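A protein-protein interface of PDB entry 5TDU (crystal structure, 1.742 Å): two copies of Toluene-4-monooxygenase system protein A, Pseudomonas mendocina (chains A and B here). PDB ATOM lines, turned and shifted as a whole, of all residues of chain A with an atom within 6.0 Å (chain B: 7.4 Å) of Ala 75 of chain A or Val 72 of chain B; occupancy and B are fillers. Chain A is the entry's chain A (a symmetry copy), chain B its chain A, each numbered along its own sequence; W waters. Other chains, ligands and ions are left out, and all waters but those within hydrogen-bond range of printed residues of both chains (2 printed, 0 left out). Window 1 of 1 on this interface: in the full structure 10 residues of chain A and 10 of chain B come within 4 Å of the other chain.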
ATOM      1  N   TYR A  70      -2.758  -0.306  -1.795  1.00  0.00           N
ATOM      2  CA  TYR A  70      -3.812  -1.039  -2.508  1.00  0.00           C
ATOM      3  C   TYR A  70      -4.501  -2.046  -1.588  1.00  0.00           C
ATOM      4  O   TYR A  70      -5.706  -2.260  -1.713  1.00  0.00           O
ATOM      5  CB  TYR A  70      -3.261  -1.746  -3.764  1.00  0.00           C
ATOM      6  CG  TYR A  70      -2.927  -0.783  -4.900  1.00  0.00           C
ATOM      7  CD1 TYR A  70      -3.930  -0.241  -5.698  1.00  0.00           C
ATOM      8  CD2 TYR A  70      -1.614  -0.407  -5.163  1.00  0.00           C
ATOM      9  CE1 TYR A  70      -3.635   0.642  -6.736  1.00  0.00           C
ATOM     10  CE2 TYR A  70      -1.306   0.480  -6.205  1.00  0.00           C
ATOM     11  CZ  TYR A  70      -2.323   1.002  -6.983  1.00  0.00           C
ATOM     12  OH  TYR A  70      -2.035   1.878  -8.006  1.00  0.00           O
ATOM     13  N   SER A  71      -3.752  -2.642  -0.658  1.00  0.00           N
ATOM     14  CA  SER A  71      -4.333  -3.608   0.283  1.00  0.00           C
ATOM     15  C   SER A  71      -5.346  -2.954   1.201  1.00  0.00           C
ATOM     16  O   SER A  71      -6.385  -3.528   1.516  1.00  0.00           O
ATOM     17  CB  SER A  71      -3.246  -4.266   1.137  1.00  0.00           C
ATOM     18  OG  SER A  71      -2.569  -5.230   0.377  1.00  0.00           O
ATOM     19  N   VAL A  72      -5.024  -1.756   1.663  1.00  0.00           N
ATOM     20  CA  VAL A  72      -5.948  -1.022   2.518  1.00  0.00           C
ATOM     21  C   VAL A  72      -7.211  -0.659   1.744  1.00  0.00           C
ATOM     22  O   VAL A  72      -8.331  -0.865   2.229  1.00  0.00           O
ATOM     23  CB  VAL A  72      -5.260   0.223   3.113  1.00  0.00           C
ATOM     24  CG1 VAL A  72      -6.271   1.126   3.796  1.00  0.00           C
ATOM     25  CG2 VAL A  72      -4.183  -0.222   4.100  1.00  0.00           C
ATOM     26  N   LYS A  73      -7.042  -0.134   0.535  1.00  0.00           N
ATOM     27  CA  LYS A  73      -8.193   0.190  -0.306  1.00  0.00           C
ATOM     28  C   LYS A  73      -9.072  -1.042  -0.491  1.00  0.00           C
ATOM     29  O   LYS A  73     -10.293  -0.969  -0.351  1.00  0.00           O
ATOM     30  CB  LYS A  73      -7.753   0.716  -1.671  1.00  0.00           C
ATOM     31  CG  LYS A  73      -8.931   1.007  -2.618  1.00  0.00           C
ATOM     32  CD  LYS A  73      -8.460   1.376  -4.013  1.00  0.00           C
ATOM     33  CE  LYS A  73      -9.626   1.728  -4.948  1.00  0.00           C
ATOM     34  NZ  LYS A  73     -10.462   0.553  -5.367  1.00  0.00           N
ATOM     35  N   ALA A  74      -8.452  -2.176  -0.799  1.00  0.00           N
ATOM     36  CA  ALA A  74      -9.217  -3.394  -1.037  1.00  0.00           C
ATOM     37  C   ALA A  74      -9.974  -3.829   0.219  1.00  0.00           C
ATOM     38  O   ALA A  74     -11.147  -4.224   0.132  1.00  0.00           O
ATOM     39  CB  ALA A  74      -8.297  -4.525  -1.528  1.00  0.00           C
ATOM     40  N   ALA A  75      -9.314  -3.754   1.380  1.00  0.00           N
ATOM     41  CA  ALA A  75      -9.919  -4.257   2.620  1.00  0.00           C
ATOM     42  C   ALA A  75     -11.072  -3.386   3.102  1.00  0.00           C
ATOM     43  O   ALA A  75     -11.907  -3.837   3.900  1.00  0.00           O
ATOM     44  CB  ALA A  75      -8.874  -4.377   3.718  1.00  0.00           C
ATOM     45  N   LEU A  76     -11.122  -2.148   2.619  1.00  0.00           N
ATOM     46  CA  LEU A  76     -12.096  -1.175   3.119  1.00  0.00           C
ATOM     47  C   LEU A  76     -13.205  -0.836   2.111  1.00  0.00           C
ATOM     48  O   LEU A  76     -13.992   0.081   2.331  1.00  0.00           O
ATOM     49  CB  LEU A  76     -11.374   0.108   3.544  1.00  0.00           C
ATOM     50  CG  LEU A  76     -10.460  -0.004   4.766  1.00  0.00           C
ATOM     51  CD1 LEU A  76      -9.823   1.344   5.079  1.00  0.00           C
ATOM     52  CD2 LEU A  76     -11.224  -0.552   5.987  1.00  0.00           C
ATOM     53  N   GLU A  77     -13.282  -1.582   1.018  1.00  0.00           N
ATOM     54  CA  GLU A  77     -14.271  -1.292  -0.019  1.00  0.00           C
ATOM     55  C   GLU A  77     -15.702  -1.254   0.515  1.00  0.00           C
ATOM     56  O   GLU A  77     -16.529  -0.496   0.015  1.00  0.00           O
ATOM     57  CB  GLU A  77     -14.174  -2.323  -1.140  1.00  0.00           C
ATOM     58  CG  GLU A  77     -12.858  -2.304  -1.877  1.00  0.00           C
ATOM     59  CD  GLU A  77     -12.712  -1.078  -2.759  1.00  0.00           C
ATOM     60  OE1 GLU A  77     -11.702  -0.982  -3.485  1.00  0.00           O
ATOM     61  OE2 GLU A  77     -13.611  -0.212  -2.732  1.00  0.00           O
ATOM     62  N   ARG A  78     -15.993  -2.068   1.528  1.00  0.00           N
ATOM     63  CA  ARG A  78     -17.356  -2.178   2.050  1.00  0.00           C
ATOM     64  C   ARG A  78     -17.574  -1.375   3.323  1.00  0.00           C
ATOM     65  O   ARG A  78     -18.520  -1.642   4.072  1.00  0.00           O
ATOM     66  CB  ARG A  78     -17.707  -3.641   2.325  1.00  0.00           C
ATOM     67  CG  ARG A  78     -17.422  -4.584   1.163  1.00  0.00           C
ATOM     68  CD  ARG A  78     -18.272  -4.237  -0.055  1.00  0.00           C
ATOM     69  NE  ARG A  78     -19.693  -4.122   0.282  1.00  0.00           N
ATOM     70  CZ  ARG A  78     -20.528  -5.155   0.351  1.00  0.00           C
ATOM     71  NH1 ARG A  78     -20.086  -6.387   0.101  1.00  0.00           N
ATOM     72  NH2 ARG A  78     -21.802  -4.959   0.673  1.00  0.00           N
ATOM     73  N   ALA A  79     -16.714  -0.397   3.573  1.00  0.00           N
ATOM     74  CA  ALA A  79     -16.845   0.429   4.768  1.00  0.00           C
ATOM     75  C   ALA A  79     -17.937   1.495   4.616  1.00  0.00           C
ATOM     76  O   ALA A  79     -18.160   2.290   5.527  1.00  0.00           O
ATOM     77  CB  ALA A  79     -15.510   1.085   5.107  1.00  0.00           C
ATOM     78  N   ASP B  66       0.352 -12.157   3.933  1.00  0.00           N
ATOM     79  CA  ASP B  66       0.740 -11.468   5.166  1.00  0.00           C
ATOM     80  C   ASP B  66       0.921  -9.960   4.950  1.00  0.00           C
ATOM     81  O   ASP B  66       0.536  -9.155   5.807  1.00  0.00           O
ATOM     82  CB  ASP B  66       2.031 -12.067   5.745  1.00  0.00           C
ATOM     83  CG  ASP B  66       1.756 -13.194   6.736  1.00  0.00           C
ATOM     84  OD1 ASP B  66       0.578 -13.401   7.107  1.00  0.00           O
ATOM     85  OD2 ASP B  66       2.718 -13.870   7.148  1.00  0.00           O
ATOM     86  N   ALA B  67       1.503  -9.563   3.820  1.00  0.00           N
ATOM     87  CA  ALA B  67       1.717  -8.132   3.599  1.00  0.00           C
ATOM     88  C   ALA B  67       0.382  -7.393   3.722  1.00  0.00           C
ATOM     89  O   ALA B  67       0.302  -6.338   4.347  1.00  0.00           O
ATOM     90  CB  ALA B  67       2.368  -7.871   2.235  1.00  0.00           C
ATOM     91  N   GLY B  68      -0.672  -7.964   3.146  1.00  0.00           N
ATOM     92  CA  GLY B  68      -1.994  -7.376   3.251  1.00  0.00           C
ATOM     93  C   GLY B  68      -2.540  -7.350   4.673  1.00  0.00           C
ATOM     94  O   GLY B  68      -3.052  -6.336   5.142  1.00  0.00           O
ATOM     95  N   ALA B  69      -2.429  -8.471   5.369  1.00  0.00           N
ATOM     96  CA  ALA B  69      -2.950  -8.562   6.730  1.00  0.00           C
ATOM     97  C   ALA B  69      -2.296  -7.524   7.641  1.00  0.00           C
ATOM     98  O   ALA B  69      -2.987  -6.835   8.422  1.00  0.00           O
ATOM     99  CB  ALA B  69      -2.742  -9.953   7.283  1.00  0.00           C
ATOM    100  N   TYR B  70      -0.975  -7.394   7.534  1.00  0.00           N
ATOM    101  CA  TYR B  70      -0.242  -6.496   8.434  1.00  0.00           C
ATOM    102  C   TYR B  70      -0.429  -5.036   8.027  1.00  0.00           C
ATOM    103  O   TYR B  70      -0.493  -4.164   8.893  1.00  0.00           O
ATOM    104  CB  TYR B  70       1.259  -6.851   8.491  1.00  0.00           C
ATOM    105  CG  TYR B  70       1.545  -8.136   9.265  1.00  0.00           C
ATOM    106  CD1 TYR B  70       1.533  -8.152  10.656  1.00  0.00           C
ATOM    107  CD2 TYR B  70       1.812  -9.330   8.605  1.00  0.00           C
ATOM    108  CE1 TYR B  70       1.790  -9.320  11.371  1.00  0.00           C
ATOM    109  CE2 TYR B  70       2.073 -10.511   9.313  1.00  0.00           C
ATOM    110  CZ  TYR B  70       2.056 -10.497  10.696  1.00  0.00           C
ATOM    111  OH  TYR B  70       2.305 -11.652  11.405  1.00  0.00           O
ATOM    112  N   SER B  71      -0.540  -4.770   6.723  1.00  0.00           N
ATOM    113  CA  SER B  71      -0.742  -3.398   6.241  1.00  0.00           C
ATOM    114  C   SER B  71      -2.075  -2.838   6.694  1.00  0.00           C
ATOM    115  O   SER B  71      -2.186  -1.668   7.051  1.00  0.00           O
ATOM    116  CB  SER B  71      -0.675  -3.337   4.712  1.00  0.00           C
ATOM    117  OG  SER B  71       0.661  -3.416   4.296  1.00  0.00           O
ATOM    118  N   VAL B  72      -3.103  -3.670   6.644  1.00  0.00           N
ATOM    119  CA  VAL B  72      -4.420  -3.242   7.099  1.00  0.00           C
ATOM    120  C   VAL B  72      -4.397  -2.963   8.599  1.00  0.00           C
ATOM    121  O   VAL B  72      -4.889  -1.923   9.055  1.00  0.00           O
ATOM    122  CB  VAL B  72      -5.487  -4.292   6.725  1.00  0.00           C
ATOM    123  CG1 VAL B  72      -6.809  -3.987   7.406  1.00  0.00           C
ATOM    124  CG2 VAL B  72      -5.656  -4.317   5.208  1.00  0.00           C
ATOM    125  N   LYS B  73      -3.817  -3.877   9.369  1.00  0.00           N
ATOM    126  CA  LYS B  73      -3.694  -3.669  10.810  1.00  0.00           C
ATOM    127  C   LYS B  73      -2.980  -2.351  11.092  1.00  0.00           C
ATOM    128  O   LYS B  73      -3.424  -1.561  11.926  1.00  0.00           O
ATOM    129  CB  LYS B  73      -2.934  -4.816  11.475  1.00  0.00           C
ATOM    130  CG  LYS B  73      -2.719  -4.608  12.985  1.00  0.00           C
ATOM    131  CD  LYS B  73      -1.829  -5.682  13.585  1.00  0.00           C
ATOM    132  CE  LYS B  73      -1.660  -5.518  15.101  1.00  0.00           C
ATOM    133  NZ  LYS B  73      -0.802  -4.354  15.508  1.00  0.00           N
ATOM    134  N   ALA B  74      -1.875  -2.110  10.393  1.00  0.00           N
ATOM    135  CA  ALA B  74      -1.105  -0.895  10.628  1.00  0.00           C
ATOM    136  C   ALA B  74      -1.920   0.354  10.291  1.00  0.00           C
ATOM    137  O   ALA B  74      -1.887   1.339  11.044  1.00  0.00           O
ATOM    138  CB  ALA B  74       0.202  -0.917   9.817  1.00  0.00           C
ATOM    139  N   ALA B  75      -2.651   0.317   9.171  1.00  0.00           N
ATOM    140  CA  ALA B  75      -3.375   1.507   8.708  1.00  0.00           C
ATOM    141  C   ALA B  75      -4.566   1.850   9.595  1.00  0.00           C
ATOM    142  O   ALA B  75      -5.057   2.987   9.573  1.00  0.00           O
ATOM    143  CB  ALA B  75      -3.842   1.328   7.272  1.00  0.00           C
ATOM    144  N   LEU B  76      -5.023   0.875  10.375  1.00  0.00           N
ATOM    145  CA  LEU B  76      -6.248   1.041  11.160  1.00  0.00           C
ATOM    146  C   LEU B  76      -6.003   1.149  12.673  1.00  0.00           C
ATOM    147  O   LEU B  76      -6.944   1.127  13.463  1.00  0.00           O
ATOM    148  CB  LEU B  76      -7.207  -0.120  10.874  1.00  0.00           C
ATOM    149  CG  LEU B  76      -7.801  -0.173   9.465  1.00  0.00           C
ATOM    150  CD1 LEU B  76      -8.741  -1.365   9.329  1.00  0.00           C
ATOM    151  CD2 LEU B  76      -8.520   1.143   9.111  1.00  0.00           C
ATOM    152  N   GLU B  77      -4.748   1.286  13.078  1.00  0.00           N
ATOM    153  CA  GLU B  77      -4.421   1.338  14.502  1.00  0.00           C
ATOM    154  C   GLU B  77      -5.180   2.434  15.248  1.00  0.00           C
ATOM    155  O   GLU B  77      -5.505   2.273  16.422  1.00  0.00           O
ATOM    156  CB  GLU B  77      -2.921   1.541  14.689  1.00  0.00           C
ATOM    157  CG  GLU B  77      -2.079   0.404  14.165  1.00  0.00           C
ATOM    158  CD  GLU B  77      -2.191  -0.838  15.027  1.00  0.00           C
ATOM    159  OE1 GLU B  77      -1.481  -1.825  14.748  1.00  0.00           O
ATOM    160  OE2 GLU B  77      -2.986  -0.827  15.991  1.00  0.00           O
ATOM    161  N   PHE B 144      -1.555  -9.961  16.695  1.00  0.00           N
ATOM    162  CA  PHE B 144      -2.620  -8.977  16.553  1.00  0.00           C
ATOM    163  C   PHE B 144      -3.161  -8.530  17.913  1.00  0.00           C
ATOM    164  O   PHE B 144      -3.276  -7.338  18.153  1.00  0.00           O
ATOM    165  CB  PHE B 144      -3.743  -9.503  15.651  1.00  0.00           C
ATOM    166  CG  PHE B 144      -3.513  -9.220  14.188  1.00  0.00           C
ATOM    167  CD1 PHE B 144      -2.325  -9.607  13.577  1.00  0.00           C
ATOM    168  CD2 PHE B 144      -4.463  -8.547  13.431  1.00  0.00           C
ATOM    169  CE1 PHE B 144      -2.090  -9.347  12.230  1.00  0.00           C
ATOM    170  CE2 PHE B 144      -4.242  -8.278  12.074  1.00  0.00           C
ATOM    171  CZ  PHE B 144      -3.048  -8.675  11.473  1.00  0.00           C
ATOM    172  N   TYR B 218     -12.456  -3.963  10.582  1.00  0.00           N
ATOM    173  CA  TYR B 218     -11.930  -4.571   9.361  1.00  0.00           C
ATOM    174  C   TYR B 218     -10.563  -5.194   9.583  1.00  0.00           C
ATOM    175  O   TYR B 218     -10.175  -6.118   8.866  1.00  0.00           O
ATOM    176  CB  TYR B 218     -11.895  -3.547   8.230  1.00  0.00           C
ATOM    177  CG  TYR B 218     -13.283  -3.050   7.944  1.00  0.00           C
ATOM    178  CD1 TYR B 218     -14.204  -3.862   7.291  1.00  0.00           C
ATOM    179  CD2 TYR B 218     -13.705  -1.798   8.387  1.00  0.00           C
ATOM    180  CE1 TYR B 218     -15.498  -3.433   7.056  1.00  0.00           C
ATOM    181  CE2 TYR B 218     -14.996  -1.360   8.158  1.00  0.00           C
ATOM    182  CZ  TYR B 218     -15.887  -2.187   7.489  1.00  0.00           C
ATOM    183  OH  TYR B 218     -17.171  -1.765   7.247  1.00  0.00           O
ATOM    184  N   THR B 219      -9.839  -4.724  10.589  1.00  0.00           N
ATOM    185  CA  THR B 219      -8.580  -5.374  10.933  1.00  0.00           C
ATOM    186  C   THR B 219      -8.822  -6.841  11.261  1.00  0.00           C
ATOM    187  O   THR B 219      -8.091  -7.722  10.809  1.00  0.00           O
ATOM    188  CB  THR B 219      -7.900  -4.694  12.124  1.00  0.00           C
ATOM    189  OG1 THR B 219      -7.442  -3.405  11.715  1.00  0.00           O
ATOM    190  CG2 THR B 219      -6.713  -5.521  12.602  1.00  0.00           C
ATOM    191  N   PHE B 220      -9.855  -7.103  12.054  1.00  0.00           N
ATOM    192  CA  PHE B 220     -10.164  -8.474  12.457  1.00  0.00           C
ATOM    193  C   PHE B 220     -10.810  -9.270  11.322  1.00  0.00           C
ATOM    194  O   PHE B 220     -10.389 -10.394  11.031  1.00  0.00           O
ATOM    195  CB  PHE B 220     -11.069  -8.449  13.697  1.00  0.00           C
ATOM    196  CG  PHE B 220     -11.379  -9.802  14.270  1.00  0.00           C
ATOM    197  CD1 PHE B 220     -10.390 -10.560  14.877  1.00  0.00           C
ATOM    198  CD2 PHE B 220     -12.680 -10.281  14.267  1.00  0.00           C
ATOM    199  CE1 PHE B 220     -10.688 -11.804  15.433  1.00  0.00           C
ATOM    200  CE2 PHE B 220     -12.988 -11.522  14.827  1.00  0.00           C
ATOM    201  CZ  PHE B 220     -11.990 -12.281  15.408  1.00  0.00           C
ATOM    202  N   ALA B 221     -11.805  -8.687  10.661  1.00  0.00           N
ATOM    203  CA  ALA B 221     -12.490  -9.377   9.572  1.00  0.00           C
ATOM    204  C   ALA B 221     -11.494  -9.756   8.477  1.00  0.00           C
ATOM    205  O   ALA B 221     -11.510 -10.875   7.959  1.00  0.00           O
ATOM    206  CB  ALA B 221     -13.623  -8.508   9.002  1.00  0.00           C
ATOM    207  N   ASN B 222     -10.615  -8.817   8.142  1.00  0.00           N
ATOM    208  CA  ASN B 222      -9.607  -9.052   7.120  1.00  0.00           C
ATOM    209  C   ASN B 222      -8.623 -10.142   7.552  1.00  0.00           C
ATOM    210  O   ASN B 222      -8.227 -10.993   6.748  1.00  0.00           O
ATOM    211  CB  ASN B 222      -8.859  -7.757   6.796  1.00  0.00           C
ATOM    212  CG  ASN B 222      -7.973  -7.902   5.584  1.00  0.00           C
ATOM    213  OD1 ASN B 222      -8.458  -8.164   4.477  1.00  0.00           O
ATOM    214  ND2 ASN B 222      -6.668  -7.762   5.782  1.00  0.00           N
ATOM    215  N   LEU B 223      -8.229 -10.119   8.820  1.00  0.00           N
ATOM    216  CA  LEU B 223      -7.327 -11.132   9.354  1.00  0.00           C
ATOM    217  C   LEU B 223      -7.905 -12.541   9.238  1.00  0.00           C
ATOM    218  O   LEU B 223      -7.283 -13.431   8.649  1.00  0.00           O
ATOM    219  CB  LEU B 223      -7.016 -10.861  10.826  1.00  0.00           C
ATOM    220  CG  LEU B 223      -6.290 -11.993  11.556  1.00  0.00           C
ATOM    221  CD1 LEU B 223      -4.865 -12.163  11.029  1.00  0.00           C
ATOM    222  CD2 LEU B 223      -6.299 -11.725  13.067  1.00  0.00           C
HETATM  223  O   HOH W   1     -17.574   1.315   8.662  1.00  0.00           O
HETATM  224  O   HOH W   2       0.472  -5.061   1.503  1.00  0.00           O
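OH of Tyr 218 of chain B is in hydrogen-bond range of O of Arg 78 of chain A (3.5 Å).
The backbone carbonyl oxygen (O) of Ala 67 of chain B lies within hydrogen-bond range of the side-chain hydroxyl (OG) of Ser 71 of chain B.
Ser 71 of chain A touches Gly 68 of chain B. Ser 71 of chain A touches Val 72 of chain B (O to CG2, 3.8 Å). Val 72 of chain A touches Ser 71 of chain B. Ala 75 of chain B touches Val 72 of chain A (CB to CG2, 3.5 Å). CG2 of Val 72 of chain B touches CB of Ala 75 of chain A (3.5 Å). Asn 222 of chain B touches Ala 75 of chain A (OD1 to CB, 3.9 Å). Leu 76 of chain A touches Tyr 218 of chain B. Tyr 218 of chain B touches Ala 79 of chain A (OH to CA, 3.3 Å).
Printed residues of chain A within 4 Å of Val 72 of chain B: Ser 71 (3.8 Å) and Ala 75 (3.5 Å). Printed residues of chain A within 4 Å of Tyr 218 of chain B: Leu 76 (3.7 Å), Arg 78 (3.5 Å) and Ala 79 (3.3 Å). Of the printed residues of chain A, Ser 71 of chain B touches Val 72.
Of the 19 printed residues of chain B, 6 touch a printed residue of chain A. Printed residues of chain B that touch a printed residue of chain A: Gly 68, Ser 71, Val 72, Ala 75, Tyr 218 and Asn 222. Hydrophobic or aromatic side chains of chain B that line the printed part of chain A: Val 72, Ala 75 and Tyr 218. Of the 10 printed residues of chain A, 6 touch a printed residue of chain B. Hydrophobic or aromatic side chains of chain A that line the printed part of chain B: Val 72, Ala 75, Leu 76 and Ala 79. Among the printed residues, 9 pairs touch across the chains. Among the printed residues, no Asp or Glu carboxylate lies within 4 Å of a Lys or Arg side-chain nitrogen of the other chain.
Ser 71 of chain A touches Val 72 of chain B, and with the chains exchanged Val 72 of chain A touches Ser 71 of chain B. Val 72 of chain A touches Ala 75 of chain B, and with the chains exchanged Ala 75 of chain A touches Val 72 of chain B. 8 positions are printed for both chains. Of the 9 pairs that touch across the chains among the printed residues, 4 have their exchanged pair printed and touching as well.
Water W2 lies within hydrogen-bond range of the backbone carbonyl oxygen of Ala 67 of chain B, the side-chain hydroxyl of Ser 71 of chain A and the side-chain hydroxyl of Ser 71 of chain B. Water W1 bridges the backbone carbonyl oxygen of Ala 79 of chain A and the side-chain hydroxyl of Tyr 218 of chain B.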
